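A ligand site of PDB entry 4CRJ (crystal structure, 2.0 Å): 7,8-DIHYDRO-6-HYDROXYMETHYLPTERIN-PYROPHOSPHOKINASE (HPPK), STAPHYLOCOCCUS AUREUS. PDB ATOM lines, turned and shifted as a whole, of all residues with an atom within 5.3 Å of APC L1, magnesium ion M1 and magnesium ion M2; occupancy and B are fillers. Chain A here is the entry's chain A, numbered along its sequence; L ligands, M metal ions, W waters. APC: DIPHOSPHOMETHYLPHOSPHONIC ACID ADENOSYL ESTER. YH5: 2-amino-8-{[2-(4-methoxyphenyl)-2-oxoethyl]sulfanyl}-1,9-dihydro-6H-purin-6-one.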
ATOM      1  N   LEU A  74      15.525  21.432 -26.576  1.00  0.00           N
ATOM      2  CA  LEU A  74      16.863  21.295 -25.994  1.00  0.00           C
ATOM      3  C   LEU A  74      17.285  19.823 -25.883  1.00  0.00           C
ATOM      4  O   LEU A  74      18.410  19.483 -26.245  1.00  0.00           O
ATOM      5  CB  LEU A  74      16.985  21.982 -24.635  1.00  0.00           C
ATOM      6  CG  LEU A  74      18.353  21.852 -23.962  1.00  0.00           C
ATOM      7  CD1 LEU A  74      19.446  22.540 -24.773  1.00  0.00           C
ATOM      8  CD2 LEU A  74      18.343  22.413 -22.546  1.00  0.00           C
ATOM      9  N   LEU A  78      20.503  17.998 -27.639  1.00  0.00           N
ATOM     10  CA  LEU A  78      21.506  17.242 -26.881  1.00  0.00           C
ATOM     11  C   LEU A  78      21.562  15.782 -27.329  1.00  0.00           C
ATOM     12  O   LEU A  78      22.653  15.224 -27.445  1.00  0.00           O
ATOM     13  CB  LEU A  78      21.246  17.332 -25.377  1.00  0.00           C
ATOM     14  CG  LEU A  78      21.310  18.745 -24.796  1.00  0.00           C
ATOM     15  CD1 LEU A  78      20.929  18.739 -23.322  1.00  0.00           C
ATOM     16  CD2 LEU A  78      22.680  19.376 -24.994  1.00  0.00           C
ATOM     17  N   GLU A  81      23.593  15.594 -30.536  1.00  0.00           N
ATOM     18  CA  GLU A  81      25.013  15.604 -30.206  1.00  0.00           C
ATOM     19  C   GLU A  81      25.503  14.202 -29.787  1.00  0.00           C
ATOM     20  O   GLU A  81      26.584  13.759 -30.199  1.00  0.00           O
ATOM     21  CB  GLU A  81      25.317  16.626 -29.105  1.00  0.00           C
ATOM     22  CG  GLU A  81      25.122  18.065 -29.538  1.00  0.00           C
ATOM     23  CD  GLU A  81      25.359  19.048 -28.407  1.00  0.00           C
ATOM     24  OE1 GLU A  81      25.823  18.635 -27.323  1.00  0.00           O
ATOM     25  OE2 GLU A  81      25.081  20.246 -28.598  1.00  0.00           O
ATOM     26  N   ARG A  86      29.447  12.988 -29.594  1.00  0.00           N
ATOM     27  CA  ARG A  86      30.110  14.014 -28.805  1.00  0.00           C
ATOM     28  C   ARG A  86      30.446  13.414 -27.453  1.00  0.00           C
ATOM     29  O   ARG A  86      29.559  13.145 -26.649  1.00  0.00           O
ATOM     30  CB  ARG A  86      29.265  15.269 -28.629  1.00  0.00           C
ATOM     31  CG  ARG A  86      30.005  16.328 -27.829  1.00  0.00           C
ATOM     32  CD  ARG A  86      29.216  17.595 -27.648  1.00  0.00           C
ATOM     33  NE  ARG A  86      29.980  18.588 -26.893  1.00  0.00           N
ATOM     34  CZ  ARG A  86      29.571  19.824 -26.633  1.00  0.00           C
ATOM     35  NH1 ARG A  86      28.387  20.252 -27.075  1.00  0.00           N
ATOM     36  NH2 ARG A  86      30.344  20.648 -25.937  1.00  0.00           N
ATOM     37  N   LYS A  89      32.849  16.932 -23.064  1.00  0.00           N
ATOM     38  CA  LYS A  89      31.849  17.828 -22.481  1.00  0.00           C
ATOM     39  C   LYS A  89      32.454  19.107 -21.876  1.00  0.00           C
ATOM     40  O   LYS A  89      31.742  19.875 -21.209  1.00  0.00           O
ATOM     41  CB  LYS A  89      30.994  17.072 -21.454  1.00  0.00           C
ATOM     42  CG  LYS A  89      30.251  15.852 -22.029  1.00  0.00           C
ATOM     43  CD  LYS A  89      29.351  16.167 -23.224  1.00  0.00           C
ATOM     44  CE  LYS A  89      28.361  17.294 -22.956  1.00  0.00           C
ATOM     45  NZ  LYS A  89      27.219  17.304 -23.919  1.00  0.00           N
ATOM     46  N   GLU A  90      33.742  19.362 -22.116  1.00  0.00           N
ATOM     47  CA  GLU A  90      34.358  20.618 -21.692  1.00  0.00           C
ATOM     48  C   GLU A  90      33.818  21.702 -22.601  1.00  0.00           C
ATOM     49  O   GLU A  90      34.005  21.648 -23.830  1.00  0.00           O
ATOM     50  CB  GLU A  90      35.890  20.566 -21.766  1.00  0.00           C
ATOM     51  CG  GLU A  90      36.540  19.531 -20.864  1.00  0.00           C
ATOM     52  CD  GLU A  90      36.366  18.099 -21.361  1.00  0.00           C
ATOM     53  OE1 GLU A  90      36.223  17.892 -22.591  1.00  0.00           O
ATOM     54  OE2 GLU A  90      36.369  17.171 -20.520  1.00  0.00           O
ATOM     55  N   ARG A  91      33.132  22.672 -22.014  1.00  0.00           N
ATOM     56  CA  ARG A  91      32.464  23.736 -22.759  1.00  0.00           C
ATOM     57  C   ARG A  91      33.436  24.486 -23.673  1.00  0.00           C
ATOM     58  O   ARG A  91      33.085  24.891 -24.773  1.00  0.00           O
ATOM     59  CB  ARG A  91      31.794  24.728 -21.806  1.00  0.00           C
ATOM     60  CG  ARG A  91      30.653  24.143 -20.984  1.00  0.00           C
ATOM     61  CD  ARG A  91      30.131  25.172 -19.989  1.00  0.00           C
ATOM     62  NE  ARG A  91      29.565  26.327 -20.681  1.00  0.00           N
ATOM     63  CZ  ARG A  91      28.269  26.506 -20.938  1.00  0.00           C
ATOM     64  NH1 ARG A  91      27.363  25.610 -20.535  1.00  0.00           N
ATOM     65  NH2 ARG A  91      27.878  27.597 -21.587  1.00  0.00           N
ATOM     66  N   ARG A  95      34.531  19.654 -30.235  1.00  0.00           N
ATOM     67  CA  ARG A  95      33.385  18.753 -30.280  1.00  0.00           C
ATOM     68  C   ARG A  95      33.023  18.327 -31.714  1.00  0.00           C
ATOM     69  O   ARG A  95      33.133  19.125 -32.674  1.00  0.00           O
ATOM     70  CB  ARG A  95      32.159  19.362 -29.568  1.00  0.00           C
ATOM     71  CG  ARG A  95      31.464  20.526 -30.279  1.00  0.00           C
ATOM     72  CD  ARG A  95      32.307  21.799 -30.307  1.00  0.00           C
ATOM     73  NE  ARG A  95      32.725  22.183 -28.964  1.00  0.00           N
ATOM     74  CZ  ARG A  95      32.017  22.961 -28.129  1.00  0.00           C
ATOM     75  NH1 ARG A  95      30.844  23.476 -28.486  1.00  0.00           N
ATOM     76  NH2 ARG A  95      32.496  23.215 -26.909  1.00  0.00           N
ATOM     77  N   ASP A  98      27.871  20.440 -32.109  1.00  0.00           N
ATOM     78  CA  ASP A  98      27.271  21.358 -31.122  1.00  0.00           C
ATOM     79  C   ASP A  98      25.990  21.885 -31.747  1.00  0.00           C
ATOM     80  O   ASP A  98      26.003  22.364 -32.872  1.00  0.00           O
ATOM     81  CB  ASP A  98      28.237  22.507 -30.835  1.00  0.00           C
ATOM     82  CG  ASP A  98      27.723  23.460 -29.773  1.00  0.00           C
ATOM     83  OD1 ASP A  98      27.066  22.995 -28.817  1.00  0.00           O
ATOM     84  OD2 ASP A  98      27.978  24.677 -29.877  1.00  0.00           O
ATOM     85  N   VAL A  99      24.879  21.745 -31.040  1.00  0.00           N
ATOM     86  CA  VAL A  99      23.591  22.249 -31.504  1.00  0.00           C
ATOM     87  C   VAL A  99      23.041  23.195 -30.436  1.00  0.00           C
ATOM     88  O   VAL A  99      22.663  22.763 -29.343  1.00  0.00           O
ATOM     89  CB  VAL A  99      22.576  21.114 -31.731  1.00  0.00           C
ATOM     90  CG1 VAL A  99      21.275  21.643 -32.309  1.00  0.00           C
ATOM     91  CG2 VAL A  99      23.172  20.063 -32.660  1.00  0.00           C
ATOM     92  N   ASP A 100      22.988  24.475 -30.770  1.00  0.00           N
ATOM     93  CA  ASP A 100      22.597  25.528 -29.847  1.00  0.00           C
ATOM     94  C   ASP A 100      21.268  26.122 -30.283  1.00  0.00           C
ATOM     95  O   ASP A 100      21.047  26.354 -31.464  1.00  0.00           O
ATOM     96  CB  ASP A 100      23.673  26.613 -29.815  1.00  0.00           C
ATOM     97  CG  ASP A 100      24.978  26.144 -29.183  1.00  0.00           C
ATOM     98  OD1 ASP A 100      24.976  25.119 -28.478  1.00  0.00           O
ATOM     99  OD2 ASP A 100      26.028  26.792 -29.387  1.00  0.00           O
ATOM    100  N   ILE A 101      20.373  26.349 -29.320  1.00  0.00           N
ATOM    101  CA  ILE A 101      19.146  27.072 -29.621  1.00  0.00           C
ATOM    102  C   ILE A 101      19.436  28.560 -29.599  1.00  0.00           C
ATOM    103  O   ILE A 101      19.813  29.114 -28.560  1.00  0.00           O
ATOM    104  CB  ILE A 101      18.012  26.770 -28.625  1.00  0.00           C
ATOM    105  CG1 ILE A 101      17.673  25.273 -28.623  1.00  0.00           C
ATOM    106  CG2 ILE A 101      16.782  27.589 -29.003  1.00  0.00           C
ATOM    107  CD1 ILE A 101      16.808  24.834 -27.451  1.00  0.00           C
ATOM    108  N   LEU A 102      19.259  29.219 -30.740  1.00  0.00           N
ATOM    109  CA  LEU A 102      19.570  30.638 -30.872  1.00  0.00           C
ATOM    110  C   LEU A 102      18.358  31.503 -30.573  1.00  0.00           C
ATOM    111  O   LEU A 102      18.475  32.500 -29.860  1.00  0.00           O
ATOM    112  CB  LEU A 102      20.083  30.941 -32.281  1.00  0.00           C
ATOM    113  CG  LEU A 102      21.348  30.194 -32.682  1.00  0.00           C
ATOM    114  CD1 LEU A 102      21.701  30.528 -34.125  1.00  0.00           C
ATOM    115  CD2 LEU A 102      22.500  30.542 -31.757  1.00  0.00           C
ATOM    116  N   LYS A 113      20.341  26.952 -16.605  1.00  0.00           N
ATOM    117  CA  LYS A 113      20.930  26.080 -17.619  1.00  0.00           C
ATOM    118  C   LYS A 113      20.364  26.291 -19.020  1.00  0.00           C
ATOM    119  O   LYS A 113      20.591  25.467 -19.905  1.00  0.00           O
ATOM    120  CB  LYS A 113      20.721  24.620 -17.215  1.00  0.00           C
ATOM    121  CG  LYS A 113      21.545  24.169 -16.028  1.00  0.00           C
ATOM    122  CD  LYS A 113      21.170  22.744 -15.646  1.00  0.00           C
ATOM    123  CE  LYS A 113      22.283  22.051 -14.866  1.00  0.00           C
ATOM    124  NZ  LYS A 113      21.961  20.612 -14.642  1.00  0.00           N
ATOM    125  N   LEU A 114      19.604  27.364 -19.241  1.00  0.00           N
ATOM    126  CA  LEU A 114      19.024  27.603 -20.565  1.00  0.00           C
ATOM    127  C   LEU A 114      18.693  29.071 -20.750  1.00  0.00           C
ATOM    128  O   LEU A 114      17.812  29.607 -20.069  1.00  0.00           O
ATOM    129  CB  LEU A 114      17.771  26.743 -20.785  1.00  0.00           C
ATOM    130  CG  LEU A 114      17.074  26.899 -22.155  1.00  0.00           C
ATOM    131  CD1 LEU A 114      18.006  26.555 -23.309  1.00  0.00           C
ATOM    132  CD2 LEU A 114      15.833  26.038 -22.225  1.00  0.00           C
ATOM    133  N   SER A 115      19.438  29.712 -21.650  1.00  0.00           N
ATOM    134  CA  SER A 115      19.172  31.067 -22.060  1.00  0.00           C
ATOM    135  C   SER A 115      18.841  31.109 -23.557  1.00  0.00           C
ATOM    136  O   SER A 115      19.640  30.665 -24.393  1.00  0.00           O
ATOM    137  CB  SER A 115      20.375  31.973 -21.756  1.00  0.00           C
ATOM    138  OG  SER A 115      20.411  32.347 -20.389  1.00  0.00           O
ATOM    139  N   VAL A 116      17.656  31.621 -23.862  1.00  0.00           N
ATOM    140  CA  VAL A 116      17.200  31.887 -25.230  1.00  0.00           C
ATOM    141  C   VAL A 116      16.555  33.268 -25.205  1.00  0.00           C
ATOM    142  O   VAL A 116      15.762  33.542 -24.313  1.00  0.00           O
ATOM    143  CB  VAL A 116      16.142  30.874 -25.682  1.00  0.00           C
ATOM    144  CG1 VAL A 116      15.704  31.164 -27.113  1.00  0.00           C
ATOM    145  CG2 VAL A 116      16.661  29.441 -25.548  1.00  0.00           C
ATOM    146  N   HIS A 118      20.045  32.920 -27.384  1.00  0.00           N
ATOM    147  CA  HIS A 118      21.347  32.528 -26.934  1.00  0.00           C
ATOM    148  C   HIS A 118      22.082  33.788 -26.525  1.00  0.00           C
ATOM    149  O   HIS A 118      22.229  34.721 -27.330  1.00  0.00           O
ATOM    150  CB  HIS A 118      22.108  31.786 -28.041  1.00  0.00           C
ATOM    151  CG  HIS A 118      23.300  31.045 -27.537  1.00  0.00           C
ATOM    152  ND1 HIS A 118      24.487  31.675 -27.220  1.00  0.00           N
ATOM    153  CD2 HIS A 118      23.481  29.743 -27.266  1.00  0.00           C
ATOM    154  CE1 HIS A 118      25.354  30.780 -26.782  1.00  0.00           C
ATOM    155  NE2 HIS A 118      24.760  29.599 -26.793  1.00  0.00           N
ATOM    156  N   PRO A 119      22.533  33.851 -25.271  1.00  0.00           N
ATOM    157  CA  PRO A 119      22.980  35.139 -24.736  1.00  0.00           C
ATOM    158  C   PRO A 119      24.321  35.612 -25.304  1.00  0.00           C
ATOM    159  O   PRO A 119      24.697  36.762 -25.084  1.00  0.00           O
ATOM    160  CB  PRO A 119      23.085  34.877 -23.230  1.00  0.00           C
ATOM    161  CG  PRO A 119      23.300  33.420 -23.099  1.00  0.00           C
ATOM    162  CD  PRO A 119      22.721  32.749 -24.310  1.00  0.00           C
ATOM    163  N   ARG A 120      25.030  34.761 -26.043  1.00  0.00           N
ATOM    164  CA  ARG A 120      26.305  35.149 -26.635  1.00  0.00           C
ATOM    165  C   ARG A 120      26.246  35.365 -28.145  1.00  0.00           C
ATOM    166  O   ARG A 120      27.252  35.736 -28.764  1.00  0.00           O
ATOM    167  CB  ARG A 120      27.365  34.106 -26.273  1.00  0.00           C
ATOM    168  CG  ARG A 120      27.737  34.170 -24.796  1.00  0.00           C
ATOM    169  CD  ARG A 120      28.439  32.906 -24.315  1.00  0.00           C
ATOM    170  NE  ARG A 120      27.508  31.834 -23.964  1.00  0.00           N
ATOM    171  CZ  ARG A 120      26.800  31.785 -22.845  1.00  0.00           C
ATOM    172  NH1 ARG A 120      26.852  32.778 -21.951  1.00  0.00           N
ATOM    173  NH2 ARG A 120      26.005  30.744 -22.624  1.00  0.00           N
ATOM    174  N   ARG A 124      29.045  37.048 -31.781  1.00  0.00           N
ATOM    175  CA  ARG A 124      29.666  35.933 -32.511  1.00  0.00           C
ATOM    176  C   ARG A 124      29.375  36.018 -33.996  1.00  0.00           C
ATOM    177  O   ARG A 124      28.267  35.746 -34.428  1.00  0.00           O
ATOM    178  CB  ARG A 124      29.183  34.612 -31.959  1.00  0.00           C
ATOM    179  CG  ARG A 124      29.669  34.322 -30.559  1.00  0.00           C
ATOM    180  CD  ARG A 124      28.973  33.106 -30.007  1.00  0.00           C
ATOM    181  NE  ARG A 124      29.552  32.648 -28.744  1.00  0.00           N
ATOM    182  CZ  ARG A 124      29.192  31.533 -28.124  1.00  0.00           C
ATOM    183  NH1 ARG A 124      28.259  30.736 -28.635  1.00  0.00           N
ATOM    184  NH2 ARG A 124      29.764  31.223 -26.970  1.00  0.00           N
HETATM  185  PG  APC L   1      27.742  28.161 -26.086  1.00  0.00           P
HETATM  186  O1G APC L   1      27.963  28.222 -27.577  1.00  0.00           O
HETATM  187  O2G APC L   1      28.092  29.477 -25.397  1.00  0.00           O
HETATM  188  O3G APC L   1      26.401  27.613 -25.701  1.00  0.00           O
HETATM  189  PB  APC L   1      28.685  25.523 -25.859  1.00  0.00           P
HETATM  190  O1B APC L   1      27.765  25.310 -27.012  1.00  0.00           O
HETATM  191  O2B APC L   1      30.175  25.057 -26.169  1.00  0.00           O
HETATM  192  O3B APC L   1      28.808  27.110 -25.533  1.00  0.00           O
HETATM  193  PA  APC L   1      27.732  23.033 -24.461  1.00  0.00           P
HETATM  194  O1A APC L   1      27.115  22.762 -25.781  1.00  0.00           O
HETATM  195  O2A APC L   1      29.000  22.141 -24.133  1.00  0.00           O
HETATM  196  C3A APC L   1      28.129  24.781 -24.310  1.00  0.00           C
HETATM  197  O5' APC L   1      26.718  22.715 -23.273  1.00  0.00           O
HETATM  198  C5' APC L   1      25.353  22.557 -23.507  1.00  0.00           C
HETATM  199  C4' APC L   1      24.651  23.093 -22.277  1.00  0.00           C
HETATM  200  O4' APC L   1      24.534  24.523 -22.285  1.00  0.00           O
HETATM  201  C3' APC L   1      23.271  22.519 -22.302  1.00  0.00           C
HETATM  202  O3' APC L   1      23.319  21.288 -21.590  1.00  0.00           O
HETATM  203  C2' APC L   1      22.406  23.624 -21.703  1.00  0.00           C
HETATM  204  O2' APC L   1      22.078  23.311 -20.335  1.00  0.00           O
HETATM  205  C1' APC L   1      23.262  24.884 -21.778  1.00  0.00           C
HETATM  206  N9  APC L   1      22.594  25.904 -22.629  1.00  0.00           N
HETATM  207  C8  APC L   1      22.248  27.136 -22.180  1.00  0.00           C
HETATM  208  N7  APC L   1      21.639  27.853 -23.143  1.00  0.00           N
HETATM  209  C5  APC L   1      21.588  27.069 -24.243  1.00  0.00           C
HETATM  210  C6  APC L   1      21.076  27.229 -25.625  1.00  0.00           C
HETATM  211  N6  APC L   1      20.491  28.393 -25.969  1.00  0.00           N
HETATM  212  N1  APC L   1      21.227  26.175 -26.493  1.00  0.00           N
HETATM  213  C2  APC L   1      21.820  25.023 -26.114  1.00  0.00           C
HETATM  214  N3  APC L   1      22.303  24.825 -24.866  1.00  0.00           N
HETATM  215  C4  APC L   1      22.230  25.791 -23.911  1.00  0.00           C
HETATM  216  C1  YH5 L   2      31.940  27.727 -32.564  1.00  0.00           C
HETATM  217  O1  YH5 L   2      30.752  27.079 -32.743  1.00  0.00           O
HETATM  218  N1  YH5 L   2      32.165  27.358 -30.095  1.00  0.00           N
HETATM  219  S1  YH5 L   2      33.239  27.470 -27.593  1.00  0.00           S
HETATM  220  C10 YH5 L   2      34.575  31.680 -24.864  1.00  0.00           C
HETATM  221  C11 YH5 L   2      34.837  32.921 -25.406  1.00  0.00           C
HETATM  222  C12 YH5 L   2      34.375  33.226 -26.662  1.00  0.00           C
HETATM  223  C13 YH5 L   2      33.650  32.308 -27.381  1.00  0.00           C
HETATM  224  C14 YH5 L   2      36.097  33.556 -23.554  1.00  0.00           C
HETATM  225  N2  YH5 L   2      34.109  28.456 -29.963  1.00  0.00           N
HETATM  226  C2  YH5 L   2      32.537  27.820 -31.325  1.00  0.00           C
HETATM  227  O2  YH5 L   2      32.343  30.543 -28.821  1.00  0.00           O
HETATM  228  N3  YH5 L   2      34.361  29.067 -32.276  1.00  0.00           N
HETATM  229  C3  YH5 L   2      33.134  27.753 -29.307  1.00  0.00           C
HETATM  230  O3  YH5 L   2      35.566  33.942 -24.805  1.00  0.00           O
HETATM  231  C4  YH5 L   2      33.728  28.494 -31.261  1.00  0.00           C
HETATM  232  N4  YH5 L   2      32.530  28.298 -33.612  1.00  0.00           N
HETATM  233  C5  YH5 L   2      33.698  28.924 -33.423  1.00  0.00           C
HETATM  234  N5  YH5 L   2      34.265  29.492 -34.534  1.00  0.00           N
HETATM  235  C6  YH5 L   2      32.104  28.822 -27.166  1.00  0.00           C
HETATM  236  C7  YH5 L   2      32.595  30.155 -27.683  1.00  0.00           C
HETATM  237  C8  YH5 L   2      33.380  31.080 -26.838  1.00  0.00           C
HETATM  238  C9  YH5 L   2      33.837  30.745 -25.578  1.00  0.00           C
HETATM  239 MG    MG M   1      26.175  24.007 -27.152  1.00  0.00          MG
HETATM  240 MG    MG M   2      27.969  26.546 -28.795  1.00  0.00          MG
HETATM  241  O   HOH W   1      25.638  27.707 -23.232  1.00  0.00           O
HETATM  242  O   HOH W   2      28.455  27.589 -30.607  1.00  0.00           O
HETATM  243  O   HOH W   3      25.254  25.167 -25.710  1.00  0.00           O
HETATM  244  O   HOH W   4      29.803  29.038 -23.209  1.00  0.00           O
HETATM  245  O   HOH W   5      25.988  20.194 -25.404  1.00  0.00           O
HETATM  246  O   HOH W   6      31.665  27.254 -24.492  1.00  0.00           O
HETATM  247  O   HOH W   7      30.069  26.429 -28.538  1.00  0.00           O
HETATM  248  O   HOH W   8      21.301  20.608 -19.911  1.00  0.00           O
HETATM  249  O   HOH W   9      24.639  22.589 -27.188  1.00  0.00           O
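O of Lys 113 is in hydrogen-bond range of O2' of APC L1 (2.7 Å). O2A of APC L1 is in salt-bridge range of NH2 of Arg 86 (2.7 Å). O2G of APC L1 lies within salt-bridge range of NH2 of Arg 124, at 2.9 Å. N of Ile 101 lies within hydrogen-bond range of N1 of APC L1. O of Ile 101 is in hydrogen-bond range of N6 of APC L1. A ring nitrogen (NE2) of His 118 sits at hydrogen-bond distance from an oxygen (O3G) of APC L1, at 2.8 Å. The guanidinium group (NE) of Arg 120 lies within salt-bridge range of an oxygen (O2G) of APC L1 (2.8 Å). The guanidinium group (NH1) of Arg 95 lies within salt-bridge range of an oxygen (O2B) of APC L1 (2.9 Å). The backbone NH of Ser 115 lies within hydrogen-bond range of a nitrogen (N7) of APC L1 (3.2 Å). A nitrogen (N6) of APC L1 is in hydrogen-bond range of the backbone carbonyl oxygen (O) of Ser 115 (2.9 Å). The guanidinium group of Arg 91 sits at hydrogen-bond distance from an oxygen (O4') of APC L1, at 3.5 Å. NH2 of Arg 124 sits close to O2 of YH5 L2 (3.2 Å).
The guanidinium group (NH1) of Arg 86 sits close to the side-chain carboxylate (OD1) of Asp 98, 3.5 Å away. OD2 of Asp 98 sits close to NH1 of Arg 95, 3.4 Å away. NH1 of Arg 86 is in salt-bridge range of OE1 of Glu 81, at 3.0 Å. N of Arg 120 lies close to ND1 of His 118. The backbone carbonyl oxygen (O) of Leu 102 sits at hydrogen-bond distance from the backbone NH (N) of His 118 (3.0 Å). NH2 of Arg 95 is in hydrogen-bond range of O of Arg 91, 2.8 Å away.
Residues that only touch APC L1: Leu 74, Leu 78, Leu 114 and Val 116. Hydrophobic or aromatic side chains within 4 Å of APC L1: Leu 74, Leu 78, Ile 101, Leu 114, Val 116 and His 118. Within 4 Å of APC L1: Leu 74, Leu 78, Arg 86, Arg 91, Arg 95, Asp 98, Asp 100, Ile 101, Lys 113, Leu 114, Ser 115, Val 116, His 118, Arg 120 and Arg 124.
Of the 21 residues printed, 2 come within 4 Å of magnesium ion M1.
Within 4 Å of magnesium ion M2: Asp 98 and Asp 100. The nearest printed residue that does not touch magnesium ion M2 is Arg 124 (4.2 Å).
Magnesium ion M1 is bound by an oxygen (O1B) of APC L1 (2.1 Å), water W3 (2.1 Å), an oxygen (O1A) of APC L1 (2.1 Å), water W9 (2.1 Å), the side-chain carboxylate (OD1) of Asp 100 (2.1 Å) and the side-chain carboxylate (OD1) of Asp 98 (2.1 Å). Magnesium ion M1 has six donor atoms within binding distance.
Magnesium ion M2 is bound by the side-chain carboxylate (OD2) of Asp 100 (2.0 Å). Magnesium ion M2 is bound by an oxygen (O1G) of APC L1. Magnesium ion M2 is bound by water W7. Magnesium ion M2 is bound by water W2, 2.1 Å away. OD2 of Asp 98 is bound to magnesium ion M2, 2.2 Å away. O1B of APC L1 binds magnesium ion M2 (2.2 Å).
Water W9 lies within hydrogen-bond range of OE2 of Glu 81 and O of Val 99. Water W7 lies within hydrogen-bond range of O2B of APC L1, N1 of YH5 L2 and NH1 of Arg 95. Water W1 lies within hydrogen-bond range of O3G of APC L1 (2.6 Å), NH2 of Arg 91 (2.8 Å) and NH2 of Arg 120 (3.1 Å). Water W4 lies within hydrogen-bond range of an oxygen (O2G) of APC L1 (2.8 Å) and the guanidinium group of Arg 91 (2.9 Å). Water W5 lies within hydrogen-bond range of the side-chain carboxylate (OE1) of Glu 81 (2.5 Å), the guanidinium group (NH1) of Arg 86 (2.9 Å), an oxygen (O5') of APC L1 (3.4 Å) and the side-chain amino group (NZ) of Lys 89 (3.5 Å).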
